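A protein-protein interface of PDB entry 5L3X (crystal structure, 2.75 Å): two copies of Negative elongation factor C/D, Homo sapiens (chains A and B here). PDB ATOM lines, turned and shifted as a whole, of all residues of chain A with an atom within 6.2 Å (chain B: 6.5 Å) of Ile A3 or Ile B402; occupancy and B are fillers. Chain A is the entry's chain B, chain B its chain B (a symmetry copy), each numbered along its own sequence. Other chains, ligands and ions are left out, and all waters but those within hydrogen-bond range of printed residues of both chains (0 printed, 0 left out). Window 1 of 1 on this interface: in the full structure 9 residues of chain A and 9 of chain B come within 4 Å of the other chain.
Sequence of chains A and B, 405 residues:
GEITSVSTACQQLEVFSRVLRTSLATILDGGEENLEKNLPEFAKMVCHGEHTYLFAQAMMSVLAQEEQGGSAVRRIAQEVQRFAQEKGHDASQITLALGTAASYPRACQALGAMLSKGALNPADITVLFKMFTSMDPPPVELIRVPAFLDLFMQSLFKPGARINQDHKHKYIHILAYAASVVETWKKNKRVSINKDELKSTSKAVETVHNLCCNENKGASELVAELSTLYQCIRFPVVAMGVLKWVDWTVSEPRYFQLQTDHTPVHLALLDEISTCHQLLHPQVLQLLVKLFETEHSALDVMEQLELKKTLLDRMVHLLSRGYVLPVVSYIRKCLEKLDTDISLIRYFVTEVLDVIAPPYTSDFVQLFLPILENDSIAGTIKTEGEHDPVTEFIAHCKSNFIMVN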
ATOM      1  N   GLY A   1       4.717  -4.050   6.492  1.00  0.00           N
ATOM      2  CA  GLY A   1       4.649  -2.781   5.792  1.00  0.00           C
ATOM      3  C   GLY A   1       4.207  -2.929   4.349  1.00  0.00           C
ATOM      4  O   GLY A   1       3.427  -2.121   3.843  1.00  0.00           O
ATOM      5  N   GLU A   2       4.711  -3.963   3.682  1.00  0.00           N
ATOM      6  CA  GLU A   2       4.345  -4.230   2.294  1.00  0.00           C
ATOM      7  C   GLU A   2       3.074  -5.069   2.215  1.00  0.00           C
ATOM      8  O   GLU A   2       2.828  -5.925   3.064  1.00  0.00           O
ATOM      9  CB  GLU A   2       5.485  -4.935   1.554  1.00  0.00           C
ATOM     10  CG  GLU A   2       6.740  -4.093   1.367  1.00  0.00           C
ATOM     11  CD  GLU A   2       7.650  -4.114   2.582  1.00  0.00           C
ATOM     12  OE1 GLU A   2       7.408  -4.931   3.496  1.00  0.00           O
ATOM     13  OE2 GLU A   2       8.610  -3.315   2.619  1.00  0.00           O
ATOM     14  N   ILE A   3       2.272  -4.820   1.186  1.00  0.00           N
ATOM     15  CA  ILE A   3       1.026  -5.549   0.989  1.00  0.00           C
ATOM     16  C   ILE A   3       1.149  -6.480  -0.224  1.00  0.00           C
ATOM     17  O   ILE A   3       1.918  -6.213  -1.147  1.00  0.00           O
ATOM     18  CB  ILE A   3      -0.167  -4.573   0.811  1.00  0.00           C
ATOM     19  CG1 ILE A   3      -1.504  -5.296   0.989  1.00  0.00           C
ATOM     20  CG2 ILE A   3      -0.098  -3.866  -0.530  1.00  0.00           C
ATOM     21  CD1 ILE A   3      -2.707  -4.411   0.746  1.00  0.00           C
ATOM     22  N   THR A   4       0.400  -7.579  -0.205  1.00  0.00           N
ATOM     23  CA  THR A   4       0.461  -8.589  -1.259  1.00  0.00           C
ATOM     24  C   THR A   4      -0.912  -9.210  -1.497  1.00  0.00           C
ATOM     25  O   THR A   4      -1.642  -9.476  -0.545  1.00  0.00           O
ATOM     26  CB  THR A   4       1.455  -9.716  -0.902  1.00  0.00           C
ATOM     27  OG1 THR A   4       2.683  -9.148  -0.431  1.00  0.00           O
ATOM     28  CG2 THR A   4       1.729 -10.598  -2.111  1.00  0.00           C
ATOM     29  N   SER A   5      -1.264  -9.449  -2.757  1.00  0.00           N
ATOM     30  CA  SER A   5      -2.515 -10.131  -3.068  1.00  0.00           C
ATOM     31  C   SER A   5      -2.388 -11.616  -2.764  1.00  0.00           C
ATOM     32  O   SER A   5      -1.293 -12.175  -2.823  1.00  0.00           O
ATOM     33  CB  SER A   5      -2.904  -9.924  -4.533  1.00  0.00           C
ATOM     34  OG  SER A   5      -2.135 -10.751  -5.387  1.00  0.00           O
ATOM     35  N   VAL A   6      -3.511 -12.251  -2.437  1.00  0.00           N
ATOM     36  CA  VAL A   6      -3.525 -13.671  -2.097  1.00  0.00           C
ATOM     37  C   VAL A   6      -3.183 -14.532  -3.309  1.00  0.00           C
ATOM     38  O   VAL A   6      -2.399 -15.473  -3.206  1.00  0.00           O
ATOM     39  CB  VAL A   6      -4.897 -14.100  -1.536  1.00  0.00           C
ATOM     40  CG1 VAL A   6      -4.900 -15.578  -1.196  1.00  0.00           C
ATOM     41  CG2 VAL A   6      -5.251 -13.269  -0.314  1.00  0.00           C
ATOM     42  N   ALA A   9       0.626 -14.605  -4.123  1.00  0.00           N
ATOM     43  CA  ALA A   9       1.383 -15.331  -3.106  1.00  0.00           C
ATOM     44  C   ALA A   9       1.217 -16.852  -3.194  1.00  0.00           C
ATOM     45  O   ALA A   9       2.030 -17.592  -2.651  1.00  0.00           O
ATOM     46  CB  ALA A   9       0.987 -14.843  -1.717  1.00  0.00           C
ATOM     47  N   VAL A  19       6.555 -16.935   2.522  1.00  0.00           N
ATOM     48  CA  VAL A  19       5.573 -16.214   3.327  1.00  0.00           C
ATOM     49  C   VAL A  19       5.110 -17.067   4.510  1.00  0.00           C
ATOM     50  O   VAL A  19       4.910 -16.556   5.610  1.00  0.00           O
ATOM     51  CB  VAL A  19       4.352 -15.788   2.488  1.00  0.00           C
ATOM     52  CG1 VAL A  19       3.410 -14.927   3.317  1.00  0.00           C
ATOM     53  CG2 VAL A  19       4.805 -15.035   1.249  1.00  0.00           C
ATOM     54  N   SER A  23       5.388 -15.806   8.304  1.00  0.00           N
ATOM     55  CA  SER A  23       4.104 -15.684   8.984  1.00  0.00           C
ATOM     56  C   SER A  23       4.071 -16.560  10.228  1.00  0.00           C
ATOM     57  O   SER A  23       3.666 -16.110  11.299  1.00  0.00           O
ATOM     58  CB  SER A  23       2.950 -16.056   8.053  1.00  0.00           C
ATOM     59  OG  SER A  23       2.799 -15.099   7.024  1.00  0.00           O
ATOM     60  N   PRO A  40      -5.219 -13.961  10.856  1.00  0.00           N
ATOM     61  CA  PRO A  40      -5.946 -13.878   9.579  1.00  0.00           C
ATOM     62  C   PRO A  40      -5.057 -13.631   8.364  1.00  0.00           C
ATOM     63  O   PRO A  40      -5.385 -14.106   7.280  1.00  0.00           O
ATOM     64  CB  PRO A  40      -6.895 -12.695   9.793  1.00  0.00           C
ATOM     65  CG  PRO A  40      -7.045 -12.595  11.265  1.00  0.00           C
ATOM     66  CD  PRO A  40      -5.707 -12.954  11.816  1.00  0.00           C
ATOM     67  N   GLU A  41      -3.952 -12.913   8.543  1.00  0.00           N
ATOM     68  CA  GLU A  41      -3.040 -12.639   7.433  1.00  0.00           C
ATOM     69  C   GLU A  41      -2.438 -13.929   6.892  1.00  0.00           C
ATOM     70  O   GLU A  41      -2.141 -14.038   5.705  1.00  0.00           O
ATOM     71  CB  GLU A  41      -1.926 -11.684   7.864  1.00  0.00           C
ATOM     72  CG  GLU A  41      -2.429 -10.337   8.358  1.00  0.00           C
ATOM     73  CD  GLU A  41      -3.345  -9.654   7.358  1.00  0.00           C
ATOM     74  OE1 GLU A  41      -2.929  -9.489   6.194  1.00  0.00           O
ATOM     75  OE2 GLU A  41      -4.481  -9.289   7.733  1.00  0.00           O
ATOM     76  N   PHE A  42      -2.264 -14.908   7.772  1.00  0.00           N
ATOM     77  CA  PHE A  42      -1.730 -16.202   7.375  1.00  0.00           C
ATOM     78  C   PHE A  42      -2.838 -17.098   6.829  1.00  0.00           C
ATOM     79  O   PHE A  42      -2.682 -17.733   5.786  1.00  0.00           O
ATOM     80  CB  PHE A  42      -1.028 -16.866   8.560  1.00  0.00           C
ATOM     81  CG  PHE A  42      -0.496 -18.237   8.265  1.00  0.00           C
ATOM     82  CD1 PHE A  42       0.394 -18.439   7.224  1.00  0.00           C
ATOM     83  CD2 PHE A  42      -0.868 -19.323   9.044  1.00  0.00           C
ATOM     84  CE1 PHE A  42       0.893 -19.697   6.952  1.00  0.00           C
ATOM     85  CE2 PHE A  42      -0.371 -20.588   8.778  1.00  0.00           C
ATOM     86  CZ  PHE A  42       0.512 -20.774   7.731  1.00  0.00           C
ATOM     87  N   LYS A  44      -5.761 -16.421   5.455  1.00  0.00           N
ATOM     88  CA  LYS A  44      -6.305 -16.031   4.157  1.00  0.00           C
ATOM     89  C   LYS A  44      -5.491 -16.619   3.006  1.00  0.00           C
ATOM     90  O   LYS A  44      -6.050 -17.069   2.004  1.00  0.00           O
ATOM     91  CB  LYS A  44      -6.364 -14.506   4.032  1.00  0.00           C
ATOM     92  CG  LYS A  44      -7.525 -13.872   4.774  1.00  0.00           C
ATOM     93  CD  LYS A  44      -7.605 -12.378   4.513  1.00  0.00           C
ATOM     94  CE  LYS A  44      -6.409 -11.654   5.102  1.00  0.00           C
ATOM     95  NZ  LYS A  44      -6.491 -10.189   4.853  1.00  0.00           N
ATOM     96  N   MET A  45      -4.172 -16.612   3.156  1.00  0.00           N
ATOM     97  CA  MET A  45      -3.291 -17.217   2.168  1.00  0.00           C
ATOM     98  C   MET A  45      -3.496 -18.729   2.095  1.00  0.00           C
ATOM     99  O   MET A  45      -3.708 -19.287   1.018  1.00  0.00           O
ATOM    100  CB  MET A  45      -1.830 -16.908   2.496  1.00  0.00           C
ATOM    101  CG  MET A  45      -0.852 -17.345   1.423  1.00  0.00           C
ATOM    102  SD  MET A  45       0.865 -17.023   1.868  1.00  0.00           S
ATOM    103  CE  MET A  45       1.074 -18.147   3.247  1.00  0.00           C
ATOM    104  N   VAL A  46      -3.434 -19.376   3.255  1.00  0.00           N
ATOM    105  CA  VAL A  46      -3.522 -20.831   3.359  1.00  0.00           C
ATOM    106  C   VAL A  46      -4.863 -21.374   2.863  1.00  0.00           C
ATOM    107  O   VAL A  46      -4.924 -22.458   2.276  1.00  0.00           O
ATOM    108  CB  VAL A  46      -3.287 -21.285   4.820  1.00  0.00           C
ATOM    109  CG1 VAL A  46      -3.642 -22.752   5.012  1.00  0.00           C
ATOM    110  CG2 VAL A  46      -1.847 -21.029   5.216  1.00  0.00           C
ATOM    111  N   THR B 361      -3.947  -4.089  -8.392  1.00  0.00           N
ATOM    112  CA  THR B 361      -2.600  -4.470  -7.997  1.00  0.00           C
ATOM    113  C   THR B 361      -2.379  -4.092  -6.539  1.00  0.00           C
ATOM    114  O   THR B 361      -3.090  -3.242  -6.002  1.00  0.00           O
ATOM    115  CB  THR B 361      -1.538  -3.793  -8.873  1.00  0.00           C
ATOM    116  OG1 THR B 361      -1.651  -2.371  -8.749  1.00  0.00           O
ATOM    117  CG2 THR B 361      -1.723  -4.187 -10.329  1.00  0.00           C
ATOM    118  N   SER B 362      -1.397  -4.718  -5.897  1.00  0.00           N
ATOM    119  CA  SER B 362      -1.089  -4.402  -4.506  1.00  0.00           C
ATOM    120  C   SER B 362      -0.492  -3.001  -4.404  1.00  0.00           C
ATOM    121  O   SER B 362      -0.661  -2.316  -3.394  1.00  0.00           O
ATOM    122  CB  SER B 362      -0.131  -5.436  -3.911  1.00  0.00           C
ATOM    123  OG  SER B 362       1.200  -5.221  -4.349  1.00  0.00           O
ATOM    124  N   ASP B 363       0.196  -2.579  -5.460  1.00  0.00           N
ATOM    125  CA  ASP B 363       0.800  -1.253  -5.495  1.00  0.00           C
ATOM    126  C   ASP B 363      -0.261  -0.158  -5.468  1.00  0.00           C
ATOM    127  O   ASP B 363      -0.068   0.883  -4.845  1.00  0.00           O
ATOM    128  CB  ASP B 363       1.687  -1.096  -6.729  1.00  0.00           C
ATOM    129  CG  ASP B 363       3.028  -1.774  -6.565  1.00  0.00           C
ATOM    130  OD1 ASP B 363       3.067  -2.889  -6.001  1.00  0.00           O
ATOM    131  OD2 ASP B 363       4.045  -1.186  -6.989  1.00  0.00           O
ATOM    132  N   VAL B 365      -3.516  -0.640  -4.306  1.00  0.00           N
ATOM    133  CA  VAL B 365      -4.206  -0.774  -3.028  1.00  0.00           C
ATOM    134  C   VAL B 365      -3.391  -0.131  -1.903  1.00  0.00           C
ATOM    135  O   VAL B 365      -3.946   0.550  -1.040  1.00  0.00           O
ATOM    136  CB  VAL B 365      -4.493  -2.257  -2.695  1.00  0.00           C
ATOM    137  CG1 VAL B 365      -5.075  -2.393  -1.297  1.00  0.00           C
ATOM    138  CG2 VAL B 365      -5.441  -2.857  -3.727  1.00  0.00           C
ATOM    139  N   GLN B 366      -2.073  -0.315  -1.940  1.00  0.00           N
ATOM    140  CA  GLN B 366      -1.185   0.217  -0.906  1.00  0.00           C
ATOM    141  C   GLN B 366      -1.226   1.749  -0.833  1.00  0.00           C
ATOM    142  O   GLN B 366      -0.793   2.339   0.160  1.00  0.00           O
ATOM    143  CB  GLN B 366       0.252  -0.262  -1.147  1.00  0.00           C
ATOM    144  CG  GLN B 366       1.175  -0.097   0.050  1.00  0.00           C
ATOM    145  CD  GLN B 366       2.527  -0.753  -0.149  1.00  0.00           C
ATOM    146  OE1 GLN B 366       2.765  -1.427  -1.152  1.00  0.00           O
ATOM    147  NE2 GLN B 366       3.423  -0.557   0.811  1.00  0.00           N
ATOM    148  N   LEU B 369      -6.019   2.481  -0.652  1.00  0.00           N
ATOM    149  CA  LEU B 369      -6.702   2.053   0.569  1.00  0.00           C
ATOM    150  C   LEU B 369      -6.405   2.988   1.754  1.00  0.00           C
ATOM    151  O   LEU B 369      -7.328   3.351   2.468  1.00  0.00           O
ATOM    152  CB  LEU B 369      -6.353   0.602   0.937  1.00  0.00           C
ATOM    153  CG  LEU B 369      -7.219  -0.018   2.040  1.00  0.00           C
ATOM    154  CD1 LEU B 369      -8.698   0.170   1.721  1.00  0.00           C
ATOM    155  CD2 LEU B 369      -6.884  -1.494   2.216  1.00  0.00           C
ATOM    156  N   CYS B 397     -10.599  -5.559  -0.718  1.00  0.00           N
ATOM    157  CA  CYS B 397      -9.205  -5.507  -0.299  1.00  0.00           C
ATOM    158  C   CYS B 397      -8.938  -6.407   0.905  1.00  0.00           C
ATOM    159  O   CYS B 397      -7.927  -7.105   0.948  1.00  0.00           O
ATOM    160  CB  CYS B 397      -8.798  -4.070   0.025  1.00  0.00           C
ATOM    161  SG  CYS B 397      -8.684  -2.993  -1.418  1.00  0.00           S
ATOM    162  N   LYS B 398      -9.846  -6.392   1.875  1.00  0.00           N
ATOM    163  CA  LYS B 398      -9.689  -7.198   3.081  1.00  0.00           C
ATOM    164  C   LYS B 398      -9.730  -8.694   2.762  1.00  0.00           C
ATOM    165  O   LYS B 398      -9.081  -9.503   3.428  1.00  0.00           O
ATOM    166  CB  LYS B 398     -10.772  -6.845   4.103  1.00  0.00           C
ATOM    167  CG  LYS B 398     -10.647  -7.611   5.411  1.00  0.00           C
ATOM    168  CD  LYS B 398     -11.806  -7.320   6.350  1.00  0.00           C
ATOM    169  CE  LYS B 398     -11.625  -8.039   7.677  1.00  0.00           C
ATOM    170  NZ  LYS B 398     -12.748  -7.759   8.617  1.00  0.00           N
ATOM    171  N   SER B 399     -10.486  -9.046   1.729  1.00  0.00           N
ATOM    172  CA  SER B 399     -10.633 -10.435   1.310  1.00  0.00           C
ATOM    173  C   SER B 399      -9.469 -10.940   0.453  1.00  0.00           C
ATOM    174  O   SER B 399      -9.093 -12.108   0.541  1.00  0.00           O
ATOM    175  CB  SER B 399     -11.950 -10.607   0.543  1.00  0.00           C
ATOM    176  OG  SER B 399     -11.974 -11.847  -0.140  1.00  0.00           O
ATOM    177  N   ASN B 400      -8.897 -10.058  -0.363  1.00  0.00           N
ATOM    178  CA  ASN B 400      -7.950 -10.477  -1.396  1.00  0.00           C
ATOM    179  C   ASN B 400      -6.491 -10.053  -1.204  1.00  0.00           C
ATOM    180  O   ASN B 400      -5.640 -10.387  -2.028  1.00  0.00           O
ATOM    181  CB  ASN B 400      -8.429  -9.968  -2.759  1.00  0.00           C
ATOM    182  CG  ASN B 400      -9.762 -10.561  -3.167  1.00  0.00           C
ATOM    183  OD1 ASN B 400     -10.813 -10.170  -2.656  1.00  0.00           O
ATOM    184  ND2 ASN B 400      -9.726 -11.505  -4.100  1.00  0.00           N
ATOM    185  N   PHE B 401      -6.195  -9.323  -0.131  1.00  0.00           N
ATOM    186  CA  PHE B 401      -4.835  -8.820   0.067  1.00  0.00           C
ATOM    187  C   PHE B 401      -4.270  -9.089   1.460  1.00  0.00           C
ATOM    188  O   PHE B 401      -5.007  -9.168   2.442  1.00  0.00           O
ATOM    189  CB  PHE B 401      -4.782  -7.321  -0.236  1.00  0.00           C
ATOM    190  CG  PHE B 401      -4.970  -6.997  -1.689  1.00  0.00           C
ATOM    191  CD1 PHE B 401      -3.885  -6.960  -2.549  1.00  0.00           C
ATOM    192  CD2 PHE B 401      -6.232  -6.736  -2.198  1.00  0.00           C
ATOM    193  CE1 PHE B 401      -4.053  -6.664  -3.891  1.00  0.00           C
ATOM    194  CE2 PHE B 401      -6.406  -6.440  -3.539  1.00  0.00           C
ATOM    195  CZ  PHE B 401      -5.315  -6.405  -4.387  1.00  0.00           C
ATOM    196  N   ILE B 402      -2.946  -9.216   1.523  1.00  0.00           N
ATOM    197  CA  ILE B 402      -2.242  -9.644   2.728  1.00  0.00           C
ATOM    198  C   ILE B 402      -0.999  -8.794   2.986  1.00  0.00           C
ATOM    199  O   ILE B 402      -0.248  -8.489   2.059  1.00  0.00           O
ATOM    200  CB  ILE B 402      -1.815 -11.128   2.616  1.00  0.00           C
ATOM    201  CG1 ILE B 402      -3.039 -12.032   2.470  1.00  0.00           C
ATOM    202  CG2 ILE B 402      -0.977 -11.552   3.812  1.00  0.00           C
ATOM    203  CD1 ILE B 402      -2.690 -13.476   2.260  1.00  0.00           C
ATOM    204  N   MET B 403      -0.788  -8.409   4.243  1.00  0.00           N
ATOM    205  CA  MET B 403       0.437  -7.722   4.645  1.00  0.00           C
ATOM    206  C   MET B 403       1.521  -8.741   5.004  1.00  0.00           C
ATOM    207  O   MET B 403       1.231  -9.768   5.616  1.00  0.00           O
ATOM    208  CB  MET B 403       0.163  -6.784   5.826  1.00  0.00           C
ATOM    209  CG  MET B 403       1.392  -6.060   6.359  1.00  0.00           C
ATOM    210  SD  MET B 403       0.987  -4.825   7.611  1.00  0.00           S
ATOM    211  CE  MET B 403       0.045  -3.651   6.635  1.00  0.00           C
ATOM    212  N   VAL B 404       2.765  -8.464   4.621  1.00  0.00           N
ATOM    213  CA  VAL B 404       3.861  -9.396   4.881  1.00  0.00           C
ATOM    214  C   VAL B 404       4.965  -8.795   5.749  1.00  0.00           C
ATOM    215  O   VAL B 404       5.101  -7.572   5.843  1.00  0.00           O
ATOM    216  CB  VAL B 404       4.493  -9.902   3.570  1.00  0.00           C
ATOM    217  CG1 VAL B 404       3.479 -10.707   2.768  1.00  0.00           C
ATOM    218  CG2 VAL B 404       5.037  -8.737   2.751  1.00  0.00           C
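The backbone carbonyl oxygen (O) of Thr A4 is in hydrogen-bond range of the backbone NH (N) of Ile B402. NE2 of Gln B366 is in hydrogen-bond range of O of Gly A1 (3.4 Å). The backbone carbonyl oxygen of Phe B401 sits at hydrogen-bond distance from the side-chain amino group of Lys A44 (3.0 Å). OG of Ser B362 sits at hydrogen-bond distance from O of Ile A3. The side-chain carboxylate (OE1) of Glu A41 sits at hydrogen-bond distance from the backbone NH (N) of Met B403 (3.1 Å). The backbone carbonyl oxygen of Lys B398 sits at hydrogen-bond distance from the side-chain amino group of Lys A44 (3.0 Å). The backbone carbonyl oxygen of Glu A2 lies within hydrogen-bond range of the backbone NH of Val B404 (3.0 Å). The backbone NH of Val A6 lies within hydrogen-bond range of the backbone carbonyl oxygen of Asn B400, 2.9 Å away.
The side-chain hydroxyl of Ser B399 is in hydrogen-bond range of the side-chain amide oxygen of Asn B400 (3.2 Å). The side-chain hydroxyl (OG) of Ser B362 lies within hydrogen-bond range of the side-chain carboxylate (OD1) of Asp B363 (3.4 Å). The side-chain carboxylate (OE2) of Glu A41 lies within salt-bridge range of the side-chain amino group (NZ) of Lys A44 (3.6 Å).
Among the printed residues, pairs that only touch across the chains: Ser A5 with Asn B400, Thr A4 with Phe B401, Glu A41 with Ile B402, Ile A3 with Ile B402, Glu A2 with Met B403, Ser A5 with Phe B401, Met A45 with Ile B402, Gly A1 with Val B404, Val A6 with Ile B402, Thr A4 with Val B404, Ile A3 with Gln B366, Ile A3 with Phe B401, Ile A3 with Val B365 and Gly A1 with Met B403.
Printed residues of chain B within 4 Å of Ile A3: Ser B362, Val B365, Gln B366, Phe B401 and Ile B402. Ile B402 touches just these residues of chain A: Ile A3, Thr A4, Val A6, Glu A41 and Met A45. Of the printed residues of chain A, Phe B401 touches Ile A3 (3.7 Å), Thr A4 (3.3 Å), Ser A5 (3.5 Å) and Lys A44 (3.0 Å). Printed residues of chain A within 4 Å of Val B404: Gly A1, Glu A2 and Thr A4. Printed residues of chain A within 4 Å of Met B403: Gly A1, Glu A2 and Glu A41. Of the printed residues of chain A, Val B365 touches Ile A3 (3.7 Å). Printed residues of chain A within 4 Å of Asn B400: Ser A5 (3.3 Å) and Val A6 (2.9 Å). Cys B397 touches none of the printed residues of chain A. Leu B369 touches none of the printed residues of chain A. The nearest residue of chain A that does not touch Ile B402 is Glu A2 (4.1 Å).
Of the 15 printed residues of chain A, 9 touch a printed residue of chain B. Hydrophobic or aromatic side chains of chain A within 4 Å of the printed part of chain B: Ile A3, Val A6 and Met A45. Of the 14 printed residues of chain B, 9 touch a printed residue of chain A.
No position is printed for both chains. Of the 22 pairs that touch across the chains among the printed residues, none has its exchanged pair printed and touching as well.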
